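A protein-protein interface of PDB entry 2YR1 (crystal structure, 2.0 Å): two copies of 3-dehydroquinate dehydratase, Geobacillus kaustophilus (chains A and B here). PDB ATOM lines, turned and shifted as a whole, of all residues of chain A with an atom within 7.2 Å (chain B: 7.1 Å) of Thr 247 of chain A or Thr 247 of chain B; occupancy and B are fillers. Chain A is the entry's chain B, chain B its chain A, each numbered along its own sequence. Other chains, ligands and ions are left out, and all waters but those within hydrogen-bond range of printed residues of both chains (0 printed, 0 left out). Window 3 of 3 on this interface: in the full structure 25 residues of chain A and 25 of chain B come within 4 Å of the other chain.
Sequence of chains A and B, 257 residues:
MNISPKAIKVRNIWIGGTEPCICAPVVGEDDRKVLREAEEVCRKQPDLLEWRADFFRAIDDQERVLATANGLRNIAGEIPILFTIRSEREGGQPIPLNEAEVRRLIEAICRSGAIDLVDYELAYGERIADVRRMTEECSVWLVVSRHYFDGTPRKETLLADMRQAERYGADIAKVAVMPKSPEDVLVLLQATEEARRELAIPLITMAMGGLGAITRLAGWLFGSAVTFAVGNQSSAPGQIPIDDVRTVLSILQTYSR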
ATOM      1  N   ILE A  22      16.000 -14.866   4.473  1.00  0.00           N
ATOM      2  CA  ILE A  22      16.752 -13.898   5.240  1.00  0.00           C
ATOM      3  C   ILE A  22      18.131 -13.694   4.625  1.00  0.00           C
ATOM      4  O   ILE A  22      18.855 -14.657   4.323  1.00  0.00           O
ATOM      5  CB  ILE A  22      16.948 -14.341   6.687  1.00  0.00           C
ATOM      6  CG1 ILE A  22      15.588 -14.673   7.326  1.00  0.00           C
ATOM      7  CG2 ILE A  22      17.650 -13.236   7.449  1.00  0.00           C
ATOM      8  CD1 ILE A  22      15.682 -15.142   8.767  1.00  0.00           C
ATOM      9  N   PRO A 241      18.863  -8.526  14.664  1.00  0.00           N
ATOM     10  CA  PRO A 241      19.689  -9.744  14.705  1.00  0.00           C
ATOM     11  C   PRO A 241      18.918 -10.940  14.144  1.00  0.00           C
ATOM     12  O   PRO A 241      17.738 -11.136  14.454  1.00  0.00           O
ATOM     13  CB  PRO A 241      19.995  -9.905  16.192  1.00  0.00           C
ATOM     14  CG  PRO A 241      20.104  -8.478  16.649  1.00  0.00           C
ATOM     15  CD  PRO A 241      18.922  -7.805  15.952  1.00  0.00           C
ATOM     16  N   ILE A 242      19.600 -11.733  13.320  1.00  0.00           N
ATOM     17  CA  ILE A 242      19.033 -12.910  12.669  1.00  0.00           C
ATOM     18  C   ILE A 242      18.215 -13.822  13.572  1.00  0.00           C
ATOM     19  O   ILE A 242      17.121 -14.254  13.209  1.00  0.00           O
ATOM     20  CB  ILE A 242      20.152 -13.765  12.001  1.00  0.00           C
ATOM     21  CG1 ILE A 242      19.582 -15.088  11.503  1.00  0.00           C
ATOM     22  CG2 ILE A 242      21.281 -14.052  13.001  1.00  0.00           C
ATOM     23  CD1 ILE A 242      18.914 -14.989  10.169  1.00  0.00           C
ATOM     24  N   ASP A 243      18.743 -14.132  14.748  1.00  0.00           N
ATOM     25  CA  ASP A 243      18.021 -15.018  15.646  1.00  0.00           C
ATOM     26  C   ASP A 243      16.638 -14.491  16.042  1.00  0.00           C
ATOM     27  O   ASP A 243      15.672 -15.254  16.092  1.00  0.00           O
ATOM     28  CB  ASP A 243      18.877 -15.294  16.881  1.00  0.00           C
ATOM     29  CG  ASP A 243      20.085 -16.164  16.559  1.00  0.00           C
ATOM     30  OD1 ASP A 243      20.869 -16.458  17.478  1.00  0.00           O
ATOM     31  OD2 ASP A 243      20.248 -16.559  15.380  1.00  0.00           O
ATOM     32  N   ASP A 244      16.541 -13.193  16.329  1.00  0.00           N
ATOM     33  CA  ASP A 244      15.256 -12.614  16.709  1.00  0.00           C
ATOM     34  C   ASP A 244      14.274 -12.644  15.528  1.00  0.00           C
ATOM     35  O   ASP A 244      13.093 -12.953  15.694  1.00  0.00           O
ATOM     36  CB  ASP A 244      15.462 -11.196  17.247  1.00  0.00           C
ATOM     37  CG  ASP A 244      16.216 -11.188  18.579  1.00  0.00           C
ATOM     38  OD1 ASP A 244      16.036 -12.143  19.373  1.00  0.00           O
ATOM     39  OD2 ASP A 244      16.980 -10.232  18.838  1.00  0.00           O
ATOM     40  N   VAL A 245      14.759 -12.347  14.327  1.00  0.00           N
ATOM     41  CA  VAL A 245      13.900 -12.416  13.154  1.00  0.00           C
ATOM     42  C   VAL A 245      13.354 -13.848  13.024  1.00  0.00           C
ATOM     43  O   VAL A 245      12.140 -14.038  12.879  1.00  0.00           O
ATOM     44  CB  VAL A 245      14.663 -12.065  11.866  1.00  0.00           C
ATOM     45  CG1 VAL A 245      13.717 -12.189  10.656  1.00  0.00           C
ATOM     46  CG2 VAL A 245      15.243 -10.650  11.967  1.00  0.00           C
ATOM     47  N   ARG A 246      14.244 -14.846  13.097  1.00  0.00           N
ATOM     48  CA  ARG A 246      13.859 -16.267  12.992  1.00  0.00           C
ATOM     49  C   ARG A 246      12.778 -16.614  14.024  1.00  0.00           C
ATOM     50  O   ARG A 246      11.817 -17.302  13.705  1.00  0.00           O
ATOM     51  CB  ARG A 246      15.073 -17.199  13.232  1.00  0.00           C
ATOM     52  CG  ARG A 246      16.211 -17.186  12.168  1.00  0.00           C
ATOM     53  CD  ARG A 246      15.864 -17.963  10.887  1.00  0.00           C
ATOM     54  NE  ARG A 246      16.999 -18.017   9.953  1.00  0.00           N
ATOM     55  CZ  ARG A 246      16.886 -18.157   8.633  1.00  0.00           C
ATOM     56  NH1 ARG A 246      15.686 -18.260   8.080  1.00  0.00           N
ATOM     57  NH2 ARG A 246      17.970 -18.182   7.859  1.00  0.00           N
ATOM     58  N   THR A 247      12.934 -16.128  15.259  1.00  0.00           N
ATOM     59  CA  THR A 247      11.959 -16.422  16.316  1.00  0.00           C
ATOM     60  C   THR A 247      10.569 -15.902  15.936  1.00  0.00           C
ATOM     61  O   THR A 247       9.572 -16.635  16.001  1.00  0.00           O
ATOM     62  CB  THR A 247      12.403 -15.808  17.674  1.00  0.00           C
ATOM     63  OG1 THR A 247      13.657 -16.385  18.077  1.00  0.00           O
ATOM     64  CG2 THR A 247      11.346 -16.073  18.776  1.00  0.00           C
ATOM     65  N   VAL A 248      10.505 -14.641  15.524  1.00  0.00           N
ATOM     66  CA  VAL A 248       9.237 -14.034  15.129  1.00  0.00           C
ATOM     67  C   VAL A 248       8.648 -14.685  13.871  1.00  0.00           C
ATOM     68  O   VAL A 248       7.440 -14.909  13.801  1.00  0.00           O
ATOM     69  CB  VAL A 248       9.399 -12.501  14.914  1.00  0.00           C
ATOM     70  CG1 VAL A 248       8.113 -11.904  14.335  1.00  0.00           C
ATOM     71  CG2 VAL A 248       9.731 -11.827  16.252  1.00  0.00           C
ATOM     72  N   LEU A 249       9.494 -14.999  12.886  1.00  0.00           N
ATOM     73  CA  LEU A 249       9.005 -15.610  11.653  1.00  0.00           C
ATOM     74  C   LEU A 249       8.358 -16.943  11.976  1.00  0.00           C
ATOM     75  O   LEU A 249       7.294 -17.287  11.452  1.00  0.00           O
ATOM     76  CB  LEU A 249      10.147 -15.830  10.658  1.00  0.00           C
ATOM     77  CG  LEU A 249      10.762 -14.595  10.004  1.00  0.00           C
ATOM     78  CD1 LEU A 249      11.919 -15.012   9.062  1.00  0.00           C
ATOM     79  CD2 LEU A 249       9.672 -13.847   9.225  1.00  0.00           C
ATOM     80  N   SER A 250       9.010 -17.695  12.849  1.00  0.00           N
ATOM     81  CA  SER A 250       8.495 -18.997  13.253  1.00  0.00           C
ATOM     82  C   SER A 250       7.059 -18.877  13.781  1.00  0.00           C
ATOM     83  O   SER A 250       6.166 -19.596  13.353  1.00  0.00           O
ATOM     84  CB  SER A 250       9.399 -19.586  14.345  1.00  0.00           C
ATOM     85  OG  SER A 250       8.856 -20.794  14.852  1.00  0.00           O
ATOM     86  N   ILE A 251       6.860 -17.964  14.720  1.00  0.00           N
ATOM     87  CA  ILE A 251       5.554 -17.748  15.314  1.00  0.00           C
ATOM     88  C   ILE A 251       4.560 -17.210  14.281  1.00  0.00           C
ATOM     89  O   ILE A 251       3.422 -17.692  14.168  1.00  0.00           O
ATOM     90  CB  ILE A 251       5.669 -16.773  16.508  1.00  0.00           C
ATOM     91  CG1 ILE A 251       6.517 -17.428  17.608  1.00  0.00           C
ATOM     92  CG2 ILE A 251       4.270 -16.421  17.059  1.00  0.00           C
ATOM     93  CD1 ILE A 251       6.871 -16.507  18.730  1.00  0.00           C
ATOM     94  N   LEU A 252       4.986 -16.230  13.503  1.00  0.00           N
ATOM     95  CA  LEU A 252       4.091 -15.666  12.497  1.00  0.00           C
ATOM     96  C   LEU A 252       3.610 -16.729  11.498  1.00  0.00           C
ATOM     97  O   LEU A 252       2.439 -16.768  11.135  1.00  0.00           O
ATOM     98  CB  LEU A 252       4.805 -14.536  11.760  1.00  0.00           C
ATOM     99  CG  LEU A 252       3.962 -13.376  11.236  1.00  0.00           C
ATOM    100  CD1 LEU A 252       3.027 -12.857  12.326  1.00  0.00           C
ATOM    101  CD2 LEU A 252       4.909 -12.269  10.743  1.00  0.00           C
ATOM    102  N   GLN A 253       4.514 -17.599  11.055  1.00  0.00           N
ATOM    103  CA  GLN A 253       4.145 -18.635  10.101  1.00  0.00           C
ATOM    104  C   GLN A 253       3.198 -19.665  10.708  1.00  0.00           C
ATOM    105  O   GLN A 253       2.236 -20.073  10.065  1.00  0.00           O
ATOM    106  CB  GLN A 253       5.398 -19.330   9.557  1.00  0.00           C
ATOM    107  CG  GLN A 253       6.364 -18.372   8.879  1.00  0.00           C
ATOM    108  CD  GLN A 253       7.567 -19.073   8.264  1.00  0.00           C
ATOM    109  OE1 GLN A 253       7.485 -19.632   7.169  1.00  0.00           O
ATOM    110  NE2 GLN A 253       8.687 -19.047   8.970  1.00  0.00           N
ATOM    111  N   LEU B 217      -0.309  -8.945  17.059  1.00  0.00           N
ATOM    112  CA  LEU B 217       1.059  -8.800  17.533  1.00  0.00           C
ATOM    113  C   LEU B 217       1.643  -7.414  17.271  1.00  0.00           C
ATOM    114  O   LEU B 217       2.583  -7.008  17.948  1.00  0.00           O
ATOM    115  CB  LEU B 217       1.958  -9.847  16.857  1.00  0.00           C
ATOM    116  CG  LEU B 217       1.615 -11.341  16.983  1.00  0.00           C
ATOM    117  CD1 LEU B 217       2.475 -12.145  16.035  1.00  0.00           C
ATOM    118  CD2 LEU B 217       1.821 -11.815  18.422  1.00  0.00           C
ATOM    119  N   PRO B 241      -1.496 -18.084  21.492  1.00  0.00           N
ATOM    120  CA  PRO B 241      -1.145 -18.376  22.881  1.00  0.00           C
ATOM    121  C   PRO B 241      -0.367 -17.225  23.508  1.00  0.00           C
ATOM    122  O   PRO B 241       0.604 -16.698  22.941  1.00  0.00           O
ATOM    123  CB  PRO B 241      -0.318 -19.654  22.764  1.00  0.00           C
ATOM    124  CG  PRO B 241      -1.011 -20.367  21.640  1.00  0.00           C
ATOM    125  CD  PRO B 241      -1.213 -19.248  20.630  1.00  0.00           C
ATOM    126  N   ILE B 242      -0.800 -16.841  24.695  1.00  0.00           N
ATOM    127  CA  ILE B 242      -0.200 -15.739  25.405  1.00  0.00           C
ATOM    128  C   ILE B 242       1.334 -15.729  25.453  1.00  0.00           C
ATOM    129  O   ILE B 242       1.956 -14.658  25.364  1.00  0.00           O
ATOM    130  CB  ILE B 242      -0.778 -15.680  26.815  1.00  0.00           C
ATOM    131  CG1 ILE B 242      -0.261 -14.438  27.538  1.00  0.00           C
ATOM    132  CG2 ILE B 242      -0.431 -16.953  27.561  1.00  0.00           C
ATOM    133  CD1 ILE B 242      -1.021 -14.148  28.814  1.00  0.00           C
ATOM    134  N   ASP B 243       1.942 -16.905  25.578  1.00  0.00           N
ATOM    135  CA  ASP B 243       3.402 -17.004  25.635  1.00  0.00           C
ATOM    136  C   ASP B 243       4.059 -16.568  24.323  1.00  0.00           C
ATOM    137  O   ASP B 243       5.104 -15.911  24.323  1.00  0.00           O
ATOM    138  CB  ASP B 243       3.820 -18.444  25.972  1.00  0.00           C
ATOM    139  CG  ASP B 243       3.558 -18.799  27.428  1.00  0.00           C
ATOM    140  OD1 ASP B 243       3.690 -17.900  28.296  1.00  0.00           O
ATOM    141  OD2 ASP B 243       3.232 -19.975  27.706  1.00  0.00           O
ATOM    142  N   ASP B 244       3.449 -16.937  23.202  1.00  0.00           N
ATOM    143  CA  ASP B 244       3.995 -16.551  21.907  1.00  0.00           C
ATOM    144  C   ASP B 244       3.764 -15.059  21.652  1.00  0.00           C
ATOM    145  O   ASP B 244       4.590 -14.392  21.036  1.00  0.00           O
ATOM    146  CB  ASP B 244       3.395 -17.423  20.800  1.00  0.00           C
ATOM    147  CG  ASP B 244       3.782 -18.903  20.948  1.00  0.00           C
ATOM    148  OD1 ASP B 244       4.974 -19.192  21.150  1.00  0.00           O
ATOM    149  OD2 ASP B 244       2.902 -19.778  20.865  1.00  0.00           O
ATOM    150  N   VAL B 245       2.650 -14.525  22.139  1.00  0.00           N
ATOM    151  CA  VAL B 245       2.382 -13.099  21.974  1.00  0.00           C
ATOM    152  C   VAL B 245       3.461 -12.295  22.703  1.00  0.00           C
ATOM    153  O   VAL B 245       4.022 -11.344  22.147  1.00  0.00           O
ATOM    154  CB  VAL B 245       0.991 -12.730  22.521  1.00  0.00           C
ATOM    155  CG1 VAL B 245       0.799 -11.235  22.492  1.00  0.00           C
ATOM    156  CG2 VAL B 245      -0.084 -13.380  21.653  1.00  0.00           C
ATOM    157  N   ARG B 246       3.760 -12.695  23.944  1.00  0.00           N
ATOM    158  CA  ARG B 246       4.789 -12.040  24.767  1.00  0.00           C
ATOM    159  C   ARG B 246       6.158 -12.078  24.078  1.00  0.00           C
ATOM    160  O   ARG B 246       6.890 -11.092  24.065  1.00  0.00           O
ATOM    161  CB  ARG B 246       4.923 -12.736  26.137  1.00  0.00           C
ATOM    162  CG  ARG B 246       3.702 -12.650  27.044  1.00  0.00           C
ATOM    163  CD  ARG B 246       3.927 -13.498  28.299  1.00  0.00           C
ATOM    164  NE  ARG B 246       2.825 -13.447  29.258  1.00  0.00           N
ATOM    165  CZ  ARG B 246       2.372 -12.322  29.800  1.00  0.00           C
ATOM    166  NH1 ARG B 246       2.927 -11.159  29.465  1.00  0.00           N
ATOM    167  NH2 ARG B 246       1.385 -12.359  30.688  1.00  0.00           N
ATOM    168  N   THR B 247       6.500 -13.230  23.520  1.00  0.00           N
ATOM    169  CA  THR B 247       7.777 -13.398  22.822  1.00  0.00           C
ATOM    170  C   THR B 247       7.938 -12.325  21.743  1.00  0.00           C
ATOM    171  O   THR B 247       8.937 -11.597  21.704  1.00  0.00           O
ATOM    172  CB  THR B 247       7.852 -14.791  22.143  1.00  0.00           C
ATOM    173  OG1 THR B 247       7.840 -15.809  23.147  1.00  0.00           O
ATOM    174  CG2 THR B 247       9.113 -14.925  21.295  1.00  0.00           C
ATOM    175  N   VAL B 248       6.947 -12.234  20.863  1.00  0.00           N
ATOM    176  CA  VAL B 248       6.989 -11.267  19.759  1.00  0.00           C
ATOM    177  C   VAL B 248       6.949  -9.820  20.232  1.00  0.00           C
ATOM    178  O   VAL B 248       7.691  -8.957  19.730  1.00  0.00           O
ATOM    179  CB  VAL B 248       5.819 -11.541  18.765  1.00  0.00           C
ATOM    180  CG1 VAL B 248       5.783 -10.504  17.686  1.00  0.00           C
ATOM    181  CG2 VAL B 248       5.991 -12.945  18.159  1.00  0.00           C
ATOM    182  N   LEU B 249       6.084  -9.538  21.200  1.00  0.00           N
ATOM    183  CA  LEU B 249       5.978  -8.173  21.693  1.00  0.00           C
ATOM    184  C   LEU B 249       7.297  -7.672  22.220  1.00  0.00           C
ATOM    185  O   LEU B 249       7.660  -6.529  21.975  1.00  0.00           O
ATOM    186  CB  LEU B 249       4.937  -8.060  22.804  1.00  0.00           C
ATOM    187  CG  LEU B 249       3.477  -8.243  22.393  1.00  0.00           C
ATOM    188  CD1 LEU B 249       2.582  -8.052  23.627  1.00  0.00           C
ATOM    189  CD2 LEU B 249       3.125  -7.232  21.303  1.00  0.00           C
ATOM    190  N   SER B 250       8.006  -8.518  22.962  1.00  0.00           N
ATOM    191  CA  SER B 250       9.280  -8.123  23.541  1.00  0.00           C
ATOM    192  C   SER B 250      10.300  -7.797  22.451  1.00  0.00           C
ATOM    193  O   SER B 250      10.992  -6.783  22.521  1.00  0.00           O
ATOM    194  CB  SER B 250       9.799  -9.223  24.462  1.00  0.00           C
ATOM    195  OG  SER B 250       8.901  -9.408  25.550  1.00  0.00           O
ATOM    196  N   ILE B 251      10.363  -8.639  21.432  1.00  0.00           N
ATOM    197  CA  ILE B 251      11.290  -8.413  20.331  1.00  0.00           C
ATOM    198  C   ILE B 251      10.861  -7.159  19.572  1.00  0.00           C
ATOM    199  O   ILE B 251      11.647  -6.246  19.361  1.00  0.00           O
ATOM    200  CB  ILE B 251      11.294  -9.621  19.394  1.00  0.00           C
ATOM    201  CG1 ILE B 251      11.887 -10.814  20.147  1.00  0.00           C
ATOM    202  CG2 ILE B 251      12.066  -9.295  18.111  1.00  0.00           C
ATOM    203  CD1 ILE B 251      11.714 -12.129  19.457  1.00  0.00           C
ATOM    204  N   LEU B 252       9.593  -7.107  19.197  1.00  0.00           N
ATOM    205  CA  LEU B 252       9.083  -5.963  18.468  1.00  0.00           C
ATOM    206  C   LEU B 252       9.319  -4.681  19.259  1.00  0.00           C
ATOM    207  O   LEU B 252       9.682  -3.665  18.686  1.00  0.00           O
ATOM    208  CB  LEU B 252       7.587  -6.152  18.191  1.00  0.00           C
ATOM    209  CG  LEU B 252       6.936  -5.310  17.095  1.00  0.00           C
ATOM    210  CD1 LEU B 252       7.739  -5.424  15.784  1.00  0.00           C
ATOM    211  CD2 LEU B 252       5.492  -5.795  16.908  1.00  0.00           C
ATOM    212  N   GLN B 253       9.137  -4.741  20.580  1.00  0.00           N
ATOM    213  CA  GLN B 253       9.309  -3.566  21.414  1.00  0.00           C
ATOM    214  C   GLN B 253      10.732  -3.059  21.542  1.00  0.00           C
ATOM    215  O   GLN B 253      10.965  -1.845  21.479  1.00  0.00           O
ATOM    216  CB  GLN B 253       8.722  -3.810  22.804  1.00  0.00           C
ATOM    217  CG  GLN B 253       7.212  -3.702  22.807  1.00  0.00           C
ATOM    218  CD  GLN B 253       6.623  -3.670  24.188  1.00  0.00           C
ATOM    219  OE1 GLN B 253       6.519  -4.699  24.861  1.00  0.00           O
ATOM    220  NE2 GLN B 253       6.233  -2.479  24.631  1.00  0.00           N
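Among the printed residues, merely in contact across the chains: Thr 247 of chain A with Thr 247 of chain B, Ile 251 of chain A with Val 248 of chain B, Ile 251 of chain A with Thr 247 of chain B, Val 248 of chain A with Ile 251 of chain B, Leu 252 of chain A with Leu 217 of chain B, Ile 251 of chain A with Asp 244 of chain B and Asp 244 of chain A with Ile 251 of chain B.
OG1 of Thr 247 of chain B lies within hydrogen-bond range of O of Asp 243 of chain B.
The backbone carbonyl oxygen (O) of Asp 243 of chain A sits at hydrogen-bond distance from the side-chain hydroxyl (OG1) of Thr 247 of chain A.
Asp 244 of chain A touches Ile 251 of chain B, and with the chains exchanged Ile 251 of chain A touches Asp 244 of chain B.
Thr 247 of chain B touches its own counterpart, Thr 247 of chain A.
Val 248 of chain A touches Ile 251 of chain B, and with the chains exchanged Ile 251 of chain A touches Val 248 of chain B.
Ile 251 of chain A touches Thr 247 of chain B, but with the chains exchanged Thr 247 of chain A does not touch Ile 251 of chain B (4.02 Å).
13 positions are printed for both chains.
Thr 247 of chain B touches just these residues of chain A: Thr 247 and Ile 251.
Of the printed residues of chain A, Ile 251 of chain B touches Asp 244 (3.99 Å) and Val 248 (3.8 Å).
Of the printed residues of chain A, Val 248 of chain B touches Ile 251.
Of the printed residues of chain B, Asp 244 of chain A touches Ile 251.
Pro 241 of chain A touches none of the printed residues of chain B.
The nearest residue of chain A that does not touch Thr 247 of chain B is Val 248 of chain A (5.5 Å).
The nearest printed residue of chain B that does not touch Leu 252 of chain A is Val 248 of chain B (5.8 Å).
Of the 14 printed residues of chain A, 5 touch a printed residue of chain B.
Printed residues of chain A that touch a printed residue of chain B: Asp 244, Thr 247, Val 248, Ile 251 and Leu 252.
Printed residues of chain B that touch a printed residue of chain A: Leu 217, Asp 244, Thr 247, Val 248 and Ile 251.
Among the printed residues, 7 pairs touch across the chains.
Among the printed residues, no Asp or Glu carboxylate lies within 4 Å of a Lys or Arg side-chain nitrogen of the other chain.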
